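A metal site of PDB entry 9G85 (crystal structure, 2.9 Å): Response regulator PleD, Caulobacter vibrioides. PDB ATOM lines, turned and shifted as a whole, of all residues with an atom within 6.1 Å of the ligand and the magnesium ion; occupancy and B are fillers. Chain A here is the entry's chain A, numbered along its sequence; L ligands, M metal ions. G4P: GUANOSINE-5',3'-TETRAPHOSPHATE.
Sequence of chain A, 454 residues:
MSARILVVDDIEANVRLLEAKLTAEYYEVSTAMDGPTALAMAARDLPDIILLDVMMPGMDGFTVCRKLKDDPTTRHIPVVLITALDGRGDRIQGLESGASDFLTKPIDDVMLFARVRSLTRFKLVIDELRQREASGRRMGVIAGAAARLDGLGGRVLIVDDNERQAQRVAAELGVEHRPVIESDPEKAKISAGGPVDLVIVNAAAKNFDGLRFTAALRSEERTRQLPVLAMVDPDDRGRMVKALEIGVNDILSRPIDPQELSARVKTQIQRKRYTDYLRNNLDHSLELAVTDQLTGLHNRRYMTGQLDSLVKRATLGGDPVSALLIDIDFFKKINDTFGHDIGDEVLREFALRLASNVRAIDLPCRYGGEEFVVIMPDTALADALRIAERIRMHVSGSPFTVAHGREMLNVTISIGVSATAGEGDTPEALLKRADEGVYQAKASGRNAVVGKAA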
ATOM      1  N   LEU A 294      -3.865 -17.013  -6.682  1.00  0.00           N
ATOM      2  CA  LEU A 294      -5.002 -16.411  -5.983  1.00  0.00           C
ATOM      3  C   LEU A 294      -5.599 -17.382  -4.965  1.00  0.00           C
ATOM      4  O   LEU A 294      -5.630 -17.101  -3.763  1.00  0.00           O
ATOM      5  CB  LEU A 294      -6.068 -15.977  -7.006  1.00  0.00           C
ATOM      6  CG  LEU A 294      -7.368 -15.400  -6.455  1.00  0.00           C
ATOM      7  CD1 LEU A 294      -7.183 -13.966  -5.974  1.00  0.00           C
ATOM      8  CD2 LEU A 294      -8.475 -15.474  -7.493  1.00  0.00           C
ATOM      9  N   ASP A 327     -18.840 -25.303 -11.402  1.00  0.00           N
ATOM     10  CA  ASP A 327     -18.919 -23.968 -11.975  1.00  0.00           C
ATOM     11  C   ASP A 327     -19.832 -23.113 -11.108  1.00  0.00           C
ATOM     12  O   ASP A 327     -20.949 -23.509 -10.796  1.00  0.00           O
ATOM     13  CB  ASP A 327     -19.438 -24.007 -13.414  1.00  0.00           C
ATOM     14  CG  ASP A 327     -19.236 -22.708 -14.155  1.00  0.00           C
ATOM     15  OD1 ASP A 327     -18.164 -22.544 -14.769  1.00  0.00           O
ATOM     16  OD2 ASP A 327     -20.145 -21.843 -14.113  1.00  0.00           O
ATOM     17  N   ILE A 328     -19.345 -21.925 -10.723  1.00  0.00           N
ATOM     18  CA  ILE A 328     -20.117 -21.037  -9.853  1.00  0.00           C
ATOM     19  C   ILE A 328     -21.198 -20.331 -10.650  1.00  0.00           C
ATOM     20  O   ILE A 328     -20.941 -19.804 -11.747  1.00  0.00           O
ATOM     21  CB  ILE A 328     -19.189 -20.026  -9.164  1.00  0.00           C
ATOM     22  CG1 ILE A 328     -18.070 -20.759  -8.412  1.00  0.00           C
ATOM     23  CG2 ILE A 328     -19.977 -19.138  -8.208  1.00  0.00           C
ATOM     24  CD1 ILE A 328     -17.094 -19.834  -7.710  1.00  0.00           C
ATOM     25  N   ASP A 329     -22.414 -20.301 -10.114  1.00  0.00           N
ATOM     26  CA  ASP A 329     -23.557 -19.714 -10.806  1.00  0.00           C
ATOM     27  C   ASP A 329     -23.596 -18.203 -10.586  1.00  0.00           C
ATOM     28  O   ASP A 329     -23.466 -17.735  -9.448  1.00  0.00           O
ATOM     29  CB  ASP A 329     -24.860 -20.338 -10.323  1.00  0.00           C
ATOM     30  CG  ASP A 329     -24.917 -21.832 -10.534  1.00  0.00           C
ATOM     31  OD1 ASP A 329     -24.367 -22.302 -11.555  1.00  0.00           O
ATOM     32  OD2 ASP A 329     -25.514 -22.530  -9.697  1.00  0.00           O
ATOM     33  N   PHE A 330     -23.757 -17.462 -11.679  1.00  0.00           N
ATOM     34  CA  PHE A 330     -23.958 -16.007 -11.637  1.00  0.00           C
ATOM     35  C   PHE A 330     -22.775 -15.288 -10.989  1.00  0.00           C
ATOM     36  O   PHE A 330     -22.946 -14.445 -10.114  1.00  0.00           O
ATOM     37  CB  PHE A 330     -25.260 -15.661 -10.898  1.00  0.00           C
ATOM     38  CG  PHE A 330     -26.453 -16.427 -11.382  1.00  0.00           C
ATOM     39  CD1 PHE A 330     -26.726 -16.550 -12.735  1.00  0.00           C
ATOM     40  CD2 PHE A 330     -27.304 -17.030 -10.477  1.00  0.00           C
ATOM     41  CE1 PHE A 330     -27.825 -17.257 -13.168  1.00  0.00           C
ATOM     42  CE2 PHE A 330     -28.409 -17.746 -10.901  1.00  0.00           C
ATOM     43  CZ  PHE A 330     -28.665 -17.854 -12.260  1.00  0.00           C
ATOM     44  N   PHE A 331     -21.566 -15.619 -11.439  1.00  0.00           N
ATOM     45  CA  PHE A 331     -20.398 -14.968 -10.865  1.00  0.00           C
ATOM     46  C   PHE A 331     -20.236 -13.542 -11.372  1.00  0.00           C
ATOM     47  O   PHE A 331     -19.696 -12.692 -10.652  1.00  0.00           O
ATOM     48  CB  PHE A 331     -19.131 -15.774 -11.151  1.00  0.00           C
ATOM     49  CG  PHE A 331     -17.997 -15.454 -10.216  1.00  0.00           C
ATOM     50  CD1 PHE A 331     -17.877 -16.117  -8.999  1.00  0.00           C
ATOM     51  CD2 PHE A 331     -17.086 -14.456 -10.526  1.00  0.00           C
ATOM     52  CE1 PHE A 331     -16.848 -15.805  -8.127  1.00  0.00           C
ATOM     53  CE2 PHE A 331     -16.050 -14.149  -9.666  1.00  0.00           C
ATOM     54  CZ  PHE A 331     -15.932 -14.832  -8.458  1.00  0.00           C
ATOM     55  N   LYS A 332     -20.694 -13.262 -12.598  1.00  0.00           N
ATOM     56  CA  LYS A 332     -20.657 -11.898 -13.103  1.00  0.00           C
ATOM     57  C   LYS A 332     -21.393 -10.938 -12.185  1.00  0.00           C
ATOM     58  O   LYS A 332     -20.917  -9.832 -11.917  1.00  0.00           O
ATOM     59  CB  LYS A 332     -21.252 -11.837 -14.516  1.00  0.00           C
ATOM     60  CG  LYS A 332     -20.492 -12.671 -15.546  1.00  0.00           C
ATOM     61  CD  LYS A 332     -21.151 -12.603 -16.928  1.00  0.00           C
ATOM     62  CE  LYS A 332     -20.349 -13.393 -17.955  1.00  0.00           C
ATOM     63  N   LYS A 333     -22.564 -11.353 -11.678  1.00  0.00           N
ATOM     64  CA  LYS A 333     -23.339 -10.481 -10.794  1.00  0.00           C
ATOM     65  C   LYS A 333     -22.571 -10.132  -9.536  1.00  0.00           C
ATOM     66  O   LYS A 333     -22.693  -9.017  -9.005  1.00  0.00           O
ATOM     67  CB  LYS A 333     -24.669 -11.144 -10.430  1.00  0.00           C
ATOM     68  CG  LYS A 333     -25.276 -12.015 -11.523  1.00  0.00           C
ATOM     69  N   ASN A 335     -19.229  -9.796  -9.345  1.00  0.00           N
ATOM     70  CA  ASN A 335     -18.312  -8.750  -9.778  1.00  0.00           C
ATOM     71  C   ASN A 335     -19.040  -7.444 -10.039  1.00  0.00           C
ATOM     72  O   ASN A 335     -18.521  -6.361  -9.755  1.00  0.00           O
ATOM     73  CB  ASN A 335     -17.563  -9.197 -11.037  1.00  0.00           C
ATOM     74  CG  ASN A 335     -16.546 -10.277 -10.743  1.00  0.00           C
ATOM     75  OD1 ASN A 335     -15.863 -10.250  -9.728  1.00  0.00           O
ATOM     76  ND2 ASN A 335     -16.432 -11.239 -11.649  1.00  0.00           N
ATOM     77  N   ASP A 336     -20.266  -7.525 -10.559  1.00  0.00           N
ATOM     78  CA  ASP A 336     -21.037  -6.314 -10.862  1.00  0.00           C
ATOM     79  C   ASP A 336     -21.468  -5.607  -9.594  1.00  0.00           C
ATOM     80  O   ASP A 336     -21.298  -4.389  -9.467  1.00  0.00           O
ATOM     81  CB  ASP A 336     -22.264  -6.682 -11.698  1.00  0.00           C
ATOM     82  CG  ASP A 336     -21.906  -7.083 -13.108  1.00  0.00           C
ATOM     83  OD1 ASP A 336     -20.719  -6.962 -13.475  1.00  0.00           O
ATOM     84  OD2 ASP A 336     -22.813  -7.528 -13.836  1.00  0.00           O
ATOM     85  N   GLY A 339     -17.831  -5.726  -6.934  1.00  0.00           N
ATOM     86  CA  GLY A 339     -16.525  -5.380  -7.474  1.00  0.00           C
ATOM     87  C   GLY A 339     -15.659  -6.608  -7.674  1.00  0.00           C
ATOM     88  O   GLY A 339     -15.924  -7.700  -7.173  1.00  0.00           O
ATOM     89  N   HIS A 340     -14.577  -6.394  -8.427  1.00  0.00           N
ATOM     90  CA  HIS A 340     -13.715  -7.500  -8.804  1.00  0.00           C
ATOM     91  C   HIS A 340     -12.890  -8.004  -7.624  1.00  0.00           C
ATOM     92  O   HIS A 340     -12.545  -9.189  -7.576  1.00  0.00           O
ATOM     93  CB  HIS A 340     -12.801  -7.091  -9.962  1.00  0.00           C
ATOM     94  CG  HIS A 340     -12.347  -8.236 -10.816  1.00  0.00           C
ATOM     95  ND1 HIS A 340     -11.127  -8.845 -10.643  1.00  0.00           N
ATOM     96  CD2 HIS A 340     -12.947  -8.882 -11.841  1.00  0.00           C
ATOM     97  CE1 HIS A 340     -10.988  -9.818 -11.523  1.00  0.00           C
ATOM     98  NE2 HIS A 340     -12.089  -9.859 -12.268  1.00  0.00           N
ATOM     99  N   ASP A 341     -12.559  -7.126  -6.677  1.00  0.00           N
ATOM    100  CA  ASP A 341     -11.758  -7.546  -5.529  1.00  0.00           C
ATOM    101  C   ASP A 341     -12.553  -8.432  -4.588  1.00  0.00           C
ATOM    102  O   ASP A 341     -12.021  -9.400  -4.022  1.00  0.00           O
ATOM    103  CB  ASP A 341     -11.214  -6.327  -4.788  1.00  0.00           C
ATOM    104  CG  ASP A 341     -10.087  -5.654  -5.529  1.00  0.00           C
ATOM    105  OD1 ASP A 341      -9.719  -6.142  -6.617  1.00  0.00           O
ATOM    106  OD2 ASP A 341      -9.551  -4.634  -5.025  1.00  0.00           O
ATOM    107  N   ILE A 342     -13.839  -8.122  -4.388  1.00  0.00           N
ATOM    108  CA  ILE A 342     -14.687  -8.995  -3.586  1.00  0.00           C
ATOM    109  C   ILE A 342     -14.902 -10.321  -4.305  1.00  0.00           C
ATOM    110  O   ILE A 342     -14.947 -11.390  -3.675  1.00  0.00           O
ATOM    111  CB  ILE A 342     -16.023  -8.305  -3.261  1.00  0.00           C
ATOM    112  CG1 ILE A 342     -15.787  -7.084  -2.371  1.00  0.00           C
ATOM    113  CG2 ILE A 342     -16.984  -9.269  -2.585  1.00  0.00           C
ATOM    114  CD1 ILE A 342     -14.837  -7.342  -1.221  1.00  0.00           C
ATOM    115  N   GLY A 343     -15.027 -10.279  -5.632  1.00  0.00           N
ATOM    116  CA  GLY A 343     -15.069 -11.510  -6.410  1.00  0.00           C
ATOM    117  C   GLY A 343     -13.865 -12.393  -6.143  1.00  0.00           C
ATOM    118  O   GLY A 343     -13.991 -13.619  -6.025  1.00  0.00           O
ATOM    119  N   ASP A 344     -12.676 -11.786  -6.049  1.00  0.00           N
ATOM    120  CA  ASP A 344     -11.483 -12.562  -5.730  1.00  0.00           C
ATOM    121  C   ASP A 344     -11.538 -13.126  -4.316  1.00  0.00           C
ATOM    122  O   ASP A 344     -11.027 -14.229  -4.074  1.00  0.00           O
ATOM    123  CB  ASP A 344     -10.238 -11.688  -5.914  1.00  0.00           C
ATOM    124  CG  ASP A 344     -10.004 -11.305  -7.367  1.00  0.00           C
ATOM    125  OD1 ASP A 344     -10.911 -11.521  -8.188  1.00  0.00           O
ATOM    126  OD2 ASP A 344      -8.912 -10.781  -7.679  1.00  0.00           O
ATOM    127  N   LEU A 347     -13.644 -16.265  -4.498  1.00  0.00           N
ATOM    128  CA  LEU A 347     -12.899 -17.381  -5.066  1.00  0.00           C
ATOM    129  C   LEU A 347     -11.945 -17.999  -4.040  1.00  0.00           C
ATOM    130  O   LEU A 347     -11.810 -19.222  -3.979  1.00  0.00           O
ATOM    131  CB  LEU A 347     -12.128 -16.934  -6.310  1.00  0.00           C
ATOM    132  CG  LEU A 347     -12.942 -16.613  -7.560  1.00  0.00           C
ATOM    133  CD1 LEU A 347     -12.012 -16.167  -8.673  1.00  0.00           C
ATOM    134  CD2 LEU A 347     -13.766 -17.802  -8.009  1.00  0.00           C
ATOM    135  N   ARG A 366      -8.026 -25.413  -9.675  1.00  0.00           N
ATOM    136  CA  ARG A 366      -8.720 -24.336 -10.378  1.00  0.00           C
ATOM    137  C   ARG A 366      -8.608 -24.639 -11.872  1.00  0.00           C
ATOM    138  O   ARG A 366      -7.525 -24.552 -12.456  1.00  0.00           O
ATOM    139  CB  ARG A 366      -8.117 -22.980 -10.039  1.00  0.00           C
ATOM    140  CG  ARG A 366      -8.957 -21.829 -10.562  1.00  0.00           C
ATOM    141  CD  ARG A 366      -8.316 -20.489 -10.289  1.00  0.00           C
ATOM    142  NE  ARG A 366      -9.095 -19.417 -10.891  1.00  0.00           N
ATOM    143  CZ  ARG A 366      -8.856 -18.126 -10.714  1.00  0.00           C
ATOM    144  NH1 ARG A 366      -7.824 -17.709 -10.009  1.00  0.00           N
ATOM    145  NH2 ARG A 366      -9.668 -17.239 -11.287  1.00  0.00           N
ATOM    146  N   GLY A 368     -10.756 -23.386 -14.627  1.00  0.00           N
ATOM    147  CA  GLY A 368     -10.941 -22.208 -15.449  1.00  0.00           C
ATOM    148  C   GLY A 368     -10.892 -20.952 -14.600  1.00  0.00           C
ATOM    149  O   GLY A 368     -10.237 -20.900 -13.568  1.00  0.00           O
ATOM    150  N   GLY A 369     -11.605 -19.928 -15.066  1.00  0.00           N
ATOM    151  CA  GLY A 369     -11.693 -18.698 -14.307  1.00  0.00           C
ATOM    152  C   GLY A 369     -12.419 -18.895 -13.001  1.00  0.00           C
ATOM    153  O   GLY A 369     -11.815 -18.781 -11.921  1.00  0.00           O
ATOM    154  N   GLU A 370     -13.705 -19.208 -13.071  1.00  0.00           N
ATOM    155  CA  GLU A 370     -14.500 -19.536 -11.901  1.00  0.00           C
ATOM    156  C   GLU A 370     -14.973 -20.982 -11.921  1.00  0.00           C
ATOM    157  O   GLU A 370     -15.979 -21.330 -11.301  1.00  0.00           O
ATOM    158  CB  GLU A 370     -15.691 -18.579 -11.779  1.00  0.00           C
ATOM    159  CG  GLU A 370     -16.460 -18.343 -13.070  1.00  0.00           C
ATOM    160  CD  GLU A 370     -17.281 -19.540 -13.514  1.00  0.00           C
ATOM    161  OE1 GLU A 370     -18.040 -20.078 -12.682  1.00  0.00           O
ATOM    162  OE2 GLU A 370     -17.171 -19.936 -14.690  1.00  0.00           O
ATOM    163  N   LYS A 442     -26.574 -26.514 -15.954  1.00  0.00           N
ATOM    164  CA  LYS A 442     -26.864 -25.097 -16.143  1.00  0.00           C
ATOM    165  C   LYS A 442     -28.184 -24.889 -16.877  1.00  0.00           C
ATOM    166  O   LYS A 442     -28.930 -23.953 -16.578  1.00  0.00           O
ATOM    167  CB  LYS A 442     -25.728 -24.413 -16.909  1.00  0.00           C
ATOM    168  CG  LYS A 442     -24.384 -24.412 -16.219  1.00  0.00           C
ATOM    169  CD  LYS A 442     -24.316 -23.382 -15.113  1.00  0.00           C
ATOM    170  CE  LYS A 442     -22.921 -23.346 -14.496  1.00  0.00           C
ATOM    171  NZ  LYS A 442     -22.786 -22.332 -13.415  1.00  0.00           N
ATOM    172  N   ARG A 446     -30.325 -24.040 -11.921  1.00  0.00           N
ATOM    173  CA  ARG A 446     -29.014 -23.911 -11.324  1.00  0.00           C
ATOM    174  C   ARG A 446     -28.971 -24.743 -10.048  1.00  0.00           C
ATOM    175  O   ARG A 446     -29.976 -25.311  -9.625  1.00  0.00           O
ATOM    176  CB  ARG A 446     -28.661 -22.456 -11.027  1.00  0.00           C
ATOM    177  CG  ARG A 446     -28.516 -21.573 -12.264  1.00  0.00           C
ATOM    178  CD  ARG A 446     -27.339 -22.004 -13.130  1.00  0.00           C
ATOM    179  NE  ARG A 446     -27.383 -21.399 -14.461  1.00  0.00           N
ATOM    180  CZ  ARG A 446     -26.687 -20.330 -14.819  1.00  0.00           C
ATOM    181  NH1 ARG A 446     -25.879 -19.706 -13.972  1.00  0.00           N
ATOM    182  NH2 ARG A 446     -26.800 -19.876 -16.069  1.00  0.00           N
HETATM  183  PB  G4P L   1     -21.808 -17.511 -14.860  1.00  0.00           P
HETATM  184  O1B G4P L   1     -23.283 -17.650 -15.163  1.00  0.00           O
HETATM  185  O2B G4P L   1     -21.579 -16.352 -13.903  1.00  0.00           O
HETATM  186  O3B G4P L   1     -21.414 -18.811 -14.214  1.00  0.00           O
HETATM  187  O3A G4P L   1     -20.860 -17.244 -16.195  1.00  0.00           O
HETATM  188  PA  G4P L   1     -19.216 -17.310 -16.055  1.00  0.00           P
HETATM  189  O1A G4P L   1     -18.674 -18.612 -16.626  1.00  0.00           O
HETATM  190  O2A G4P L   1     -18.979 -17.255 -14.553  1.00  0.00           O
HETATM  191  O5' G4P L   1     -18.447 -16.008 -16.735  1.00  0.00           O
HETATM  192  C5' G4P L   1     -17.031 -15.884 -16.665  1.00  0.00           C
HETATM  193  C4' G4P L   1     -16.649 -15.149 -15.393  1.00  0.00           C
HETATM  194  O4' G4P L   1     -15.722 -15.713 -14.709  1.00  0.00           O
HETATM  195  C3' G4P L   1     -16.058 -13.635 -15.780  1.00  0.00           C
HETATM  196  O3' G4P L   1     -17.146 -12.740 -16.327  1.00  0.00           O
HETATM  197  C2' G4P L   1     -15.605 -13.229 -14.722  1.00  0.00           C
HETATM  198  O2' G4P L   1     -16.606 -12.392 -13.981  1.00  0.00           O
HETATM  199  C1' G4P L   1     -15.376 -14.528 -13.804  1.00  0.00           C
HETATM  200  N9  G4P L   1     -14.181 -14.435 -13.228  1.00  0.00           N
HETATM  201  C8  G4P L   1     -13.486 -15.334 -13.954  1.00  0.00           C
HETATM  202  N7  G4P L   1     -12.213 -15.325 -13.418  1.00  0.00           N
HETATM  203  C5  G4P L   1     -12.193 -14.440 -12.405  1.00  0.00           C
HETATM  204  C6  G4P L   1     -11.145 -13.927 -11.394  1.00  0.00           C
HETATM  205  O6  G4P L   1     -10.036 -14.364 -11.428  1.00  0.00           O
HETATM  206  N1  G4P L   1     -11.452 -12.929 -10.394  1.00  0.00           N
HETATM  207  C2  G4P L   1     -12.786 -12.392 -10.320  1.00  0.00           C
HETATM  208  N2  G4P L   1     -13.225 -11.391  -9.368  1.00  0.00           N
HETATM  209  N3  G4P L   1     -13.773 -12.861 -11.282  1.00  0.00           N
HETATM  210  C4  G4P L   1     -13.440 -13.890 -12.306  1.00  0.00           C
HETATM  211  PC  G4P L   1     -16.848 -11.099 -16.576  1.00  0.00           P
HETATM  212  O1C G4P L   1     -17.397 -10.626 -17.911  1.00  0.00           O
HETATM  213  O2C G4P L   1     -17.523 -10.332 -15.469  1.00  0.00           O
HETATM  214  O3C G4P L   1     -15.199 -10.816 -16.466  1.00  0.00           O
HETATM  215  PD  G4P L   1     -14.560  -9.729 -15.372  1.00  0.00           P
HETATM  216  O1D G4P L   1     -13.069  -9.943 -15.190  1.00  0.00           O
HETATM  217  O2D G4P L   1     -15.280  -9.942 -14.055  1.00  0.00           O
HETATM  218  O3D G4P L   1     -14.809  -8.319 -15.864  1.00  0.00           O
HETATM  219 MG    MG M   1     -19.929 -19.848 -13.723  1.00  0.00          MG
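The magnesium ion is bound by O3B of the ligand, OD2 of Asp 327, OE1 of Glu 370 and O of Ile 328.
The magnesium ion has four donor atoms within binding distance.
Lys 442 touches the magnesium ion (NZ to MG, 3.8 Å).
Four residues have an atom within 4 Å of the magnesium ion: Asp 327, Ile 328, Glu 370 and Lys 442.
Along chain A the residues within 4 Å of the magnesium ion span positions 327 to 442.
The nearest printed residue that does not touch the magnesium ion is Asp 329 (4.4 Å).
N of Phe 331 is in hydrogen-bond range of O2B of the ligand, 2.6 Å away.
OD1 of Asp 344 lies within hydrogen-bond range of N2 of the ligand, at 2.6 Å.
ND2 of Asn 335 is in hydrogen-bond range of O2' of the ligand, at 2.6 Å.
NH2 of Arg 366 is in hydrogen-bond range of O6 of the ligand (2.9 Å).
The backbone carbonyl oxygen of His 340 lies within hydrogen-bond range of a nitrogen (N2) of the ligand.
NE2 of His 340 lies within hydrogen-bond range of O1D of the ligand (3.1 Å).
An oxygen (O2B) of the ligand sits close to the backbone NH of Phe 330 (3.3 Å).
The backbone NH of Lys 332 lies within hydrogen-bond range of an oxygen (O2B) of the ligand (3.5 Å).
The guanidinium group of Arg 446 is in salt-bridge range of an oxygen (O1B) of the ligand, 3.5 Å away.
The side-chain amino group (NZ) of Lys 442 sits close to an oxygen (O3B) of the ligand (3.9 Å).
Merely in contact with the ligand: Gly 343 (3.4 Å), Leu 347 (3.6 Å) and Gly 369 (3.5 Å).
15 residues have an atom within 4 Å of the ligand: Asp 327, Ile 328, Phe 330, Phe 331, Lys 332, Asn 335, His 340, Gly 343, Asp 344, Leu 347, Arg 366, Gly 369, Glu 370, Lys 442 and Arg 446.
The nearest printed residue that does not touch the ligand is Asp 329 (4.1 Å).
NZ of Lys 442 lies within hydrogen-bond range of O of Asp 327 (3.4 Å).
The guanidinium group (NH2) of Arg 366 lies within hydrogen-bond range of the backbone carbonyl oxygen (O) of Gly 369.
The backbone carbonyl oxygen (O) of Gly 368 sits at hydrogen-bond distance from the guanidinium group (NE) of Arg 366 (3.3 Å).
NH1 of Arg 446 is in salt-bridge range of OD1 of Asp 329 (3.9 Å).
The side-chain carboxylate (OD1) of Asp 329 lies within salt-bridge range of the side-chain amino group (NZ) of Lys 442 (2.4 Å).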
